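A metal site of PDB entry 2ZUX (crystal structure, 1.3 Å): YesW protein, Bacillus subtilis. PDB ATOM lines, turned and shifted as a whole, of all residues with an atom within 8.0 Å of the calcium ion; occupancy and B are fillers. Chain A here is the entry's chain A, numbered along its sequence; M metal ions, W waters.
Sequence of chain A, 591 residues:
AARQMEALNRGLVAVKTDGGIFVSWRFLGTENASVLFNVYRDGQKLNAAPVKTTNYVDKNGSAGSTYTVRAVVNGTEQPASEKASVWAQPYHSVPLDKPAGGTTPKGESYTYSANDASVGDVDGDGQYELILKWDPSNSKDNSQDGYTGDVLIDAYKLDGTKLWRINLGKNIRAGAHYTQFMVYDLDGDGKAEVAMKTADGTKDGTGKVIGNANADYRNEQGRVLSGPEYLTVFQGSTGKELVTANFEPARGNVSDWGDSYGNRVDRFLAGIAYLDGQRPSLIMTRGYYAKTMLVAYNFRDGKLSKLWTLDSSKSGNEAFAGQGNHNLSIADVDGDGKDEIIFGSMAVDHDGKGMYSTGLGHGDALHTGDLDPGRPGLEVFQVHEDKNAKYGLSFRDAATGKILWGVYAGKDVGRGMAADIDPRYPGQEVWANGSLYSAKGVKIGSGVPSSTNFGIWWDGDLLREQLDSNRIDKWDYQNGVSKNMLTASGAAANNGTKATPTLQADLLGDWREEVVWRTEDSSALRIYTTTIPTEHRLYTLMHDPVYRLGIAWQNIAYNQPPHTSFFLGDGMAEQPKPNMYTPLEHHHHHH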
ATOM      1  N   LEU A 371     -24.193   5.042 -15.351  1.00  0.00           N
ATOM      2  CA  LEU A 371     -23.606   4.624 -14.094  1.00  0.00           C
ATOM      3  C   LEU A 371     -24.037   5.546 -12.969  1.00  0.00           C
ATOM      4  O   LEU A 371     -24.289   5.107 -11.841  1.00  0.00           O
ATOM      5  CB  LEU A 371     -22.075   4.576 -14.213  1.00  0.00           C
ATOM      6  CG  LEU A 371     -21.453   3.853 -15.425  1.00  0.00           C
ATOM      7  CD1 LEU A 371     -19.916   3.818 -15.342  1.00  0.00           C
ATOM      8  CD2 LEU A 371     -22.013   2.437 -15.575  1.00  0.00           C
ATOM      9  N   PRO A 373     -27.068   7.885 -12.475  1.00  0.00           N
ATOM     10  CA  PRO A 373     -28.348   8.327 -13.019  1.00  0.00           C
ATOM     11  C   PRO A 373     -28.735   9.748 -12.576  1.00  0.00           C
ATOM     12  O   PRO A 373     -29.670  10.332 -13.136  1.00  0.00           O
ATOM     13  CB  PRO A 373     -29.328   7.274 -12.475  1.00  0.00           C
ATOM     14  CG  PRO A 373     -28.723   6.814 -11.214  1.00  0.00           C
ATOM     15  CD  PRO A 373     -27.230   6.839 -11.442  1.00  0.00           C
ATOM     16  N   ALA A 419     -21.647  -2.066 -11.475  1.00  0.00           N
ATOM     17  CA  ALA A 419     -22.953  -2.691 -11.246  1.00  0.00           C
ATOM     18  C   ALA A 419     -23.614  -2.076 -10.024  1.00  0.00           C
ATOM     19  O   ALA A 419     -22.948  -1.738  -9.054  1.00  0.00           O
ATOM     20  CB  ALA A 419     -22.813  -4.194 -11.058  1.00  0.00           C
ATOM     21  N   ASP A 420     -24.936  -1.948 -10.079  1.00  0.00           N
ATOM     22  CA  ASP A 420     -25.688  -1.532  -8.903  1.00  0.00           C
ATOM     23  C   ASP A 420     -25.789  -2.725  -7.962  1.00  0.00           C
ATOM     24  O   ASP A 420     -26.609  -3.621  -8.171  1.00  0.00           O
ATOM     25  CB  ASP A 420     -27.088  -1.042  -9.272  1.00  0.00           C
ATOM     26  CG  ASP A 420     -27.814  -0.430  -8.082  1.00  0.00           C
ATOM     27  OD1 ASP A 420     -27.189  -0.303  -7.004  1.00  0.00           O
ATOM     28  OD2 ASP A 420     -29.006  -0.065  -8.220  1.00  0.00           O
ATOM     29  N   ILE A 421     -24.926  -2.720  -6.938  1.00  0.00           N
ATOM     30  CA  ILE A 421     -24.898  -3.806  -5.958  1.00  0.00           C
ATOM     31  C   ILE A 421     -25.285  -3.349  -4.560  1.00  0.00           C
ATOM     32  O   ILE A 421     -25.489  -4.176  -3.669  1.00  0.00           O
ATOM     33  CB  ILE A 421     -23.515  -4.508  -5.931  1.00  0.00           C
ATOM     34  CG1 ILE A 421     -22.413  -3.587  -5.357  1.00  0.00           C
ATOM     35  CG2 ILE A 421     -23.142  -5.008  -7.324  1.00  0.00           C
ATOM     36  CD1 ILE A 421     -21.081  -4.270  -5.188  1.00  0.00           C
ATOM     37  N   ASP A 422     -25.390  -2.034  -4.360  1.00  0.00           N
ATOM     38  CA  ASP A 422     -25.644  -1.466  -3.041  1.00  0.00           C
ATOM     39  C   ASP A 422     -26.733  -0.413  -3.196  1.00  0.00           C
ATOM     40  O   ASP A 422     -26.504   0.624  -3.809  1.00  0.00           O
ATOM     41  CB  ASP A 422     -24.353  -0.854  -2.494  1.00  0.00           C
ATOM     42  CG  ASP A 422     -24.467  -0.428  -1.035  1.00  0.00           C
ATOM     43  OD1 ASP A 422     -25.591  -0.121  -0.582  1.00  0.00           O
ATOM     44  OD2 ASP A 422     -23.417  -0.402  -0.372  1.00  0.00           O
ATOM     45  N   PRO A 423     -27.931  -0.667  -2.656  1.00  0.00           N
ATOM     46  CA  PRO A 423     -29.036   0.282  -2.849  1.00  0.00           C
ATOM     47  C   PRO A 423     -28.934   1.534  -1.962  1.00  0.00           C
ATOM     48  O   PRO A 423     -29.738   2.451  -2.117  1.00  0.00           O
ATOM     49  CB  PRO A 423     -30.268  -0.541  -2.473  1.00  0.00           C
ATOM     50  CG  PRO A 423     -29.776  -1.488  -1.452  1.00  0.00           C
ATOM     51  CD  PRO A 423     -28.348  -1.823  -1.843  1.00  0.00           C
ATOM     52  N   ARG A 424     -27.949   1.562  -1.068  1.00  0.00           N
ATOM     53  CA  ARG A 424     -27.779   2.712  -0.181  1.00  0.00           C
ATOM     54  C   ARG A 424     -27.094   3.873  -0.912  1.00  0.00           C
ATOM     55  O   ARG A 424     -27.120   5.005  -0.439  1.00  0.00           O
ATOM     56  CB  ARG A 424     -26.988   2.327   1.060  1.00  0.00           C
ATOM     57  CG  ARG A 424     -27.596   1.172   1.849  1.00  0.00           C
ATOM     58  CD  ARG A 424     -26.647   0.685   2.922  1.00  0.00           C
ATOM     59  NE  ARG A 424     -25.369   0.263   2.349  1.00  0.00           N
ATOM     60  CZ  ARG A 424     -24.271   0.027   3.055  1.00  0.00           C
ATOM     61  NH1 ARG A 424     -24.281   0.142   4.383  1.00  0.00           N
ATOM     62  NH2 ARG A 424     -23.146  -0.336   2.443  1.00  0.00           N
ATOM     63  N   TYR A 425     -26.489   3.580  -2.062  1.00  0.00           N
ATOM     64  CA  TYR A 425     -25.870   4.607  -2.875  1.00  0.00           C
ATOM     65  C   TYR A 425     -26.553   4.604  -4.237  1.00  0.00           C
ATOM     66  O   TYR A 425     -26.508   3.584  -4.942  1.00  0.00           O
ATOM     67  CB  TYR A 425     -24.369   4.360  -3.032  1.00  0.00           C
ATOM     68  CG  TYR A 425     -23.600   4.449  -1.737  1.00  0.00           C
ATOM     69  CD1 TYR A 425     -22.969   5.633  -1.366  1.00  0.00           C
ATOM     70  CD2 TYR A 425     -23.518   3.358  -0.873  1.00  0.00           C
ATOM     71  CE1 TYR A 425     -22.254   5.729  -0.172  1.00  0.00           C
ATOM     72  CE2 TYR A 425     -22.802   3.435   0.314  1.00  0.00           C
ATOM     73  CZ  TYR A 425     -22.182   4.629   0.653  1.00  0.00           C
ATOM     74  OH  TYR A 425     -21.475   4.696   1.835  1.00  0.00           O
ATOM     75  N   PRO A 426     -27.213   5.705  -4.608  1.00  0.00           N
ATOM     76  CA  PRO A 426     -27.895   5.723  -5.898  1.00  0.00           C
ATOM     77  C   PRO A 426     -26.937   5.419  -7.043  1.00  0.00           C
ATOM     78  O   PRO A 426     -25.762   5.813  -7.002  1.00  0.00           O
ATOM     79  CB  PRO A 426     -28.438   7.155  -6.000  1.00  0.00           C
ATOM     80  CG  PRO A 426     -28.585   7.589  -4.570  1.00  0.00           C
ATOM     81  CD  PRO A 426     -27.411   6.972  -3.873  1.00  0.00           C
ATOM     82  N   GLY A 427     -27.429   4.697  -8.036  1.00  0.00           N
ATOM     83  CA  GLY A 427     -26.648   4.408  -9.218  1.00  0.00           C
ATOM     84  C   GLY A 427     -25.798   3.159  -9.097  1.00  0.00           C
ATOM     85  O   GLY A 427     -25.949   2.364  -8.168  1.00  0.00           O
ATOM     86  N   GLN A 428     -24.940   2.974 -10.094  1.00  0.00           N
ATOM     87  CA  GLN A 428     -24.071   1.816 -10.135  1.00  0.00           C
ATOM     88  C   GLN A 428     -22.807   2.070  -9.337  1.00  0.00           C
ATOM     89  O   GLN A 428     -22.156   3.091  -9.500  1.00  0.00           O
ATOM     90  CB  GLN A 428     -23.713   1.490 -11.588  1.00  0.00           C
ATOM     91  CG  GLN A 428     -24.929   1.194 -12.450  1.00  0.00           C
ATOM     92  CD  GLN A 428     -24.556   0.534 -13.761  1.00  0.00           C
ATOM     93  OE1 GLN A 428     -23.775  -0.414 -13.786  1.00  0.00           O
ATOM     94  NE2 GLN A 428     -25.126   1.027 -14.849  1.00  0.00           N
ATOM     95  N   GLU A 429     -22.487   1.114  -8.479  1.00  0.00           N
ATOM     96  CA  GLU A 429     -21.187   1.088  -7.823  1.00  0.00           C
ATOM     97  C   GLU A 429     -20.127   0.635  -8.808  1.00  0.00           C
ATOM     98  O   GLU A 429     -20.422   0.028  -9.848  1.00  0.00           O
ATOM     99  CB  GLU A 429     -21.234   0.124  -6.631  1.00  0.00           C
ATOM    100  CG  GLU A 429     -22.022   0.654  -5.420  1.00  0.00           C
ATOM    101  CD  GLU A 429     -23.506   0.872  -5.691  1.00  0.00           C
ATOM    102  OE1 GLU A 429     -24.210  -0.097  -6.095  1.00  0.00           O
ATOM    103  OE2 GLU A 429     -23.990   2.012  -5.507  1.00  0.00           O
ATOM    104  N   VAL A 430     -18.877   0.951  -8.496  1.00  0.00           N
ATOM    105  CA  VAL A 430     -17.751   0.491  -9.311  1.00  0.00           C
ATOM    106  C   VAL A 430     -16.681  -0.033  -8.377  1.00  0.00           C
ATOM    107  O   VAL A 430     -16.571   0.410  -7.226  1.00  0.00           O
ATOM    108  CB  VAL A 430     -17.186   1.586 -10.251  1.00  0.00           C
ATOM    109  CG1 VAL A 430     -18.269   2.088 -11.218  1.00  0.00           C
ATOM    110  CG2 VAL A 430     -16.604   2.736  -9.458  1.00  0.00           C
ATOM    111  N   TYR A 437     -16.546   1.608  -4.734  1.00  0.00           N
ATOM    112  CA  TYR A 437     -16.916   3.020  -4.715  1.00  0.00           C
ATOM    113  C   TYR A 437     -18.331   3.250  -5.191  1.00  0.00           C
ATOM    114  O   TYR A 437     -18.858   2.500  -6.028  1.00  0.00           O
ATOM    115  CB  TYR A 437     -15.994   3.822  -5.648  1.00  0.00           C
ATOM    116  CG  TYR A 437     -14.527   3.706  -5.372  1.00  0.00           C
ATOM    117  CD1 TYR A 437     -13.874   4.629  -4.540  1.00  0.00           C
ATOM    118  CD2 TYR A 437     -13.769   2.692  -5.946  1.00  0.00           C
ATOM    119  CE1 TYR A 437     -12.511   4.531  -4.300  1.00  0.00           C
ATOM    120  CE2 TYR A 437     -12.417   2.573  -5.706  1.00  0.00           C
ATOM    121  CZ  TYR A 437     -11.790   3.500  -4.892  1.00  0.00           C
ATOM    122  OH  TYR A 437     -10.445   3.384  -4.663  1.00  0.00           O
ATOM    123  N   SER A 438     -18.945   4.317  -4.708  1.00  0.00           N
ATOM    124  CA  SER A 438     -20.195   4.779  -5.281  1.00  0.00           C
ATOM    125  C   SER A 438     -19.908   5.415  -6.642  1.00  0.00           C
ATOM    126  O   SER A 438     -18.754   5.663  -6.990  1.00  0.00           O
ATOM    127  CB  SER A 438     -20.839   5.811  -4.372  1.00  0.00           C
ATOM    128  OG  SER A 438     -20.164   7.054  -4.470  1.00  0.00           O
ATOM    129  N   ALA A 439     -20.971   5.686  -7.391  1.00  0.00           N
ATOM    130  CA  ALA A 439     -20.849   6.378  -8.677  1.00  0.00           C
ATOM    131  C   ALA A 439     -20.211   7.770  -8.544  1.00  0.00           C
ATOM    132  O   ALA A 439     -19.743   8.342  -9.533  1.00  0.00           O
ATOM    133  CB  ALA A 439     -22.216   6.487  -9.339  1.00  0.00           C
ATOM    134  N   ILE A 444     -16.807   2.741  -0.345  1.00  0.00           N
ATOM    135  CA  ILE A 444     -17.821   2.079   0.462  1.00  0.00           C
ATOM    136  C   ILE A 444     -17.176   0.929   1.238  1.00  0.00           C
ATOM    137  O   ILE A 444     -16.680  -0.026   0.646  1.00  0.00           O
ATOM    138  CB  ILE A 444     -18.953   1.499  -0.418  1.00  0.00           C
ATOM    139  CG1 ILE A 444     -19.602   2.606  -1.263  1.00  0.00           C
ATOM    140  CG2 ILE A 444     -19.987   0.747   0.442  1.00  0.00           C
ATOM    141  CD1 ILE A 444     -20.483   2.078  -2.390  1.00  0.00           C
ATOM    142  N   LEU A 463     -31.105  -4.964  -8.419  1.00  0.00           N
ATOM    143  CA  LEU A 463     -29.651  -4.942  -8.257  1.00  0.00           C
ATOM    144  C   LEU A 463     -29.038  -5.945  -9.232  1.00  0.00           C
ATOM    145  O   LEU A 463     -29.734  -6.865  -9.694  1.00  0.00           O
ATOM    146  CB  LEU A 463     -29.248  -5.286  -6.814  1.00  0.00           C
ATOM    147  CG  LEU A 463     -29.773  -4.346  -5.723  1.00  0.00           C
ATOM    148  CD1 LEU A 463     -29.365  -4.863  -4.365  1.00  0.00           C
ATOM    149  CD2 LEU A 463     -29.277  -2.911  -5.925  1.00  0.00           C
ATOM    150  N   PHE A 567     -30.459   3.576 -16.826  1.00  0.00           N
ATOM    151  CA  PHE A 567     -30.129   3.043 -15.529  1.00  0.00           C
ATOM    152  C   PHE A 567     -31.151   1.980 -15.131  1.00  0.00           C
ATOM    153  O   PHE A 567     -32.323   2.292 -14.910  1.00  0.00           O
ATOM    154  CB  PHE A 567     -30.049   4.132 -14.449  1.00  0.00           C
ATOM    155  CG  PHE A 567     -29.889   3.589 -13.065  1.00  0.00           C
ATOM    156  CD1 PHE A 567     -28.696   2.974 -12.688  1.00  0.00           C
ATOM    157  CD2 PHE A 567     -30.939   3.656 -12.152  1.00  0.00           C
ATOM    158  CE1 PHE A 567     -28.556   2.432 -11.419  1.00  0.00           C
ATOM    159  CE2 PHE A 567     -30.792   3.120 -10.868  1.00  0.00           C
ATOM    160  CZ  PHE A 567     -29.593   2.511 -10.509  1.00  0.00           C
ATOM    161  N   GLY A 569     -31.717  -0.429 -12.202  1.00  0.00           N
ATOM    162  CA  GLY A 569     -31.252  -0.671 -10.851  1.00  0.00           C
ATOM    163  C   GLY A 569     -32.221  -0.179  -9.814  1.00  0.00           C
ATOM    164  O   GLY A 569     -33.330   0.261 -10.155  1.00  0.00           O
ATOM    165  N   ASP A 570     -31.813  -0.248  -8.558  1.00  0.00           N
ATOM    166  CA  ASP A 570     -32.679   0.167  -7.460  1.00  0.00           C
ATOM    167  C   ASP A 570     -32.987   1.643  -7.576  1.00  0.00           C
ATOM    168  O   ASP A 570     -32.094   2.466  -7.782  1.00  0.00           O
ATOM    169  CB  ASP A 570     -32.037  -0.139  -6.119  1.00  0.00           C
ATOM    170  CG  ASP A 570     -32.968   0.141  -4.962  1.00  0.00           C
ATOM    171  OD1 ASP A 570     -33.886  -0.677  -4.741  1.00  0.00           O
ATOM    172  OD2 ASP A 570     -32.798   1.186  -4.315  1.00  0.00           O
HETATM  173 CA    CA M   1     -26.317   1.558  -5.969  1.00  0.00          CA
HETATM  174  O   HOH W   1     -28.647   1.947  -6.313  1.00  0.00           O
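The backbone carbonyl oxygen (O) of Glu 429 lies within hydrogen-bond range of the backbone NH (N) of Ala 419 (2.9 Å). The guanidinium group (NH2) of Arg 424 lies within salt-bridge range of the side-chain carboxylate (OD2) of Asp 422. N of Ile 421 lies close to OE1 of Glu 429, 2.8 Å away. The side-chain carboxylate of Asp 420 lies within hydrogen-bond range of the backbone NH of Asp 570, at 2.8 Å.
O of Tyr 425 binds the calcium ion (2.3 Å). OD1 of Asp 420 binds the calcium ion, 2.3 Å away. The calcium ion is bound by O of Asp 422 (2.4 Å). The backbone carbonyl oxygen (O) of Gly 427 is bound to the calcium ion (2.4 Å). The calcium ion is bound by water W1 (2.4 Å). The calcium ion is bound by the side-chain carboxylate (OE2) of Glu 429. The calcium ion is bound by OE1 of Glu 429 (2.7 Å).
Water W1 lies within hydrogen-bond range of the side-chain carboxylate of Asp 420 (2.8 Å) and the backbone NH of Gly 427 (3.5 Å).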
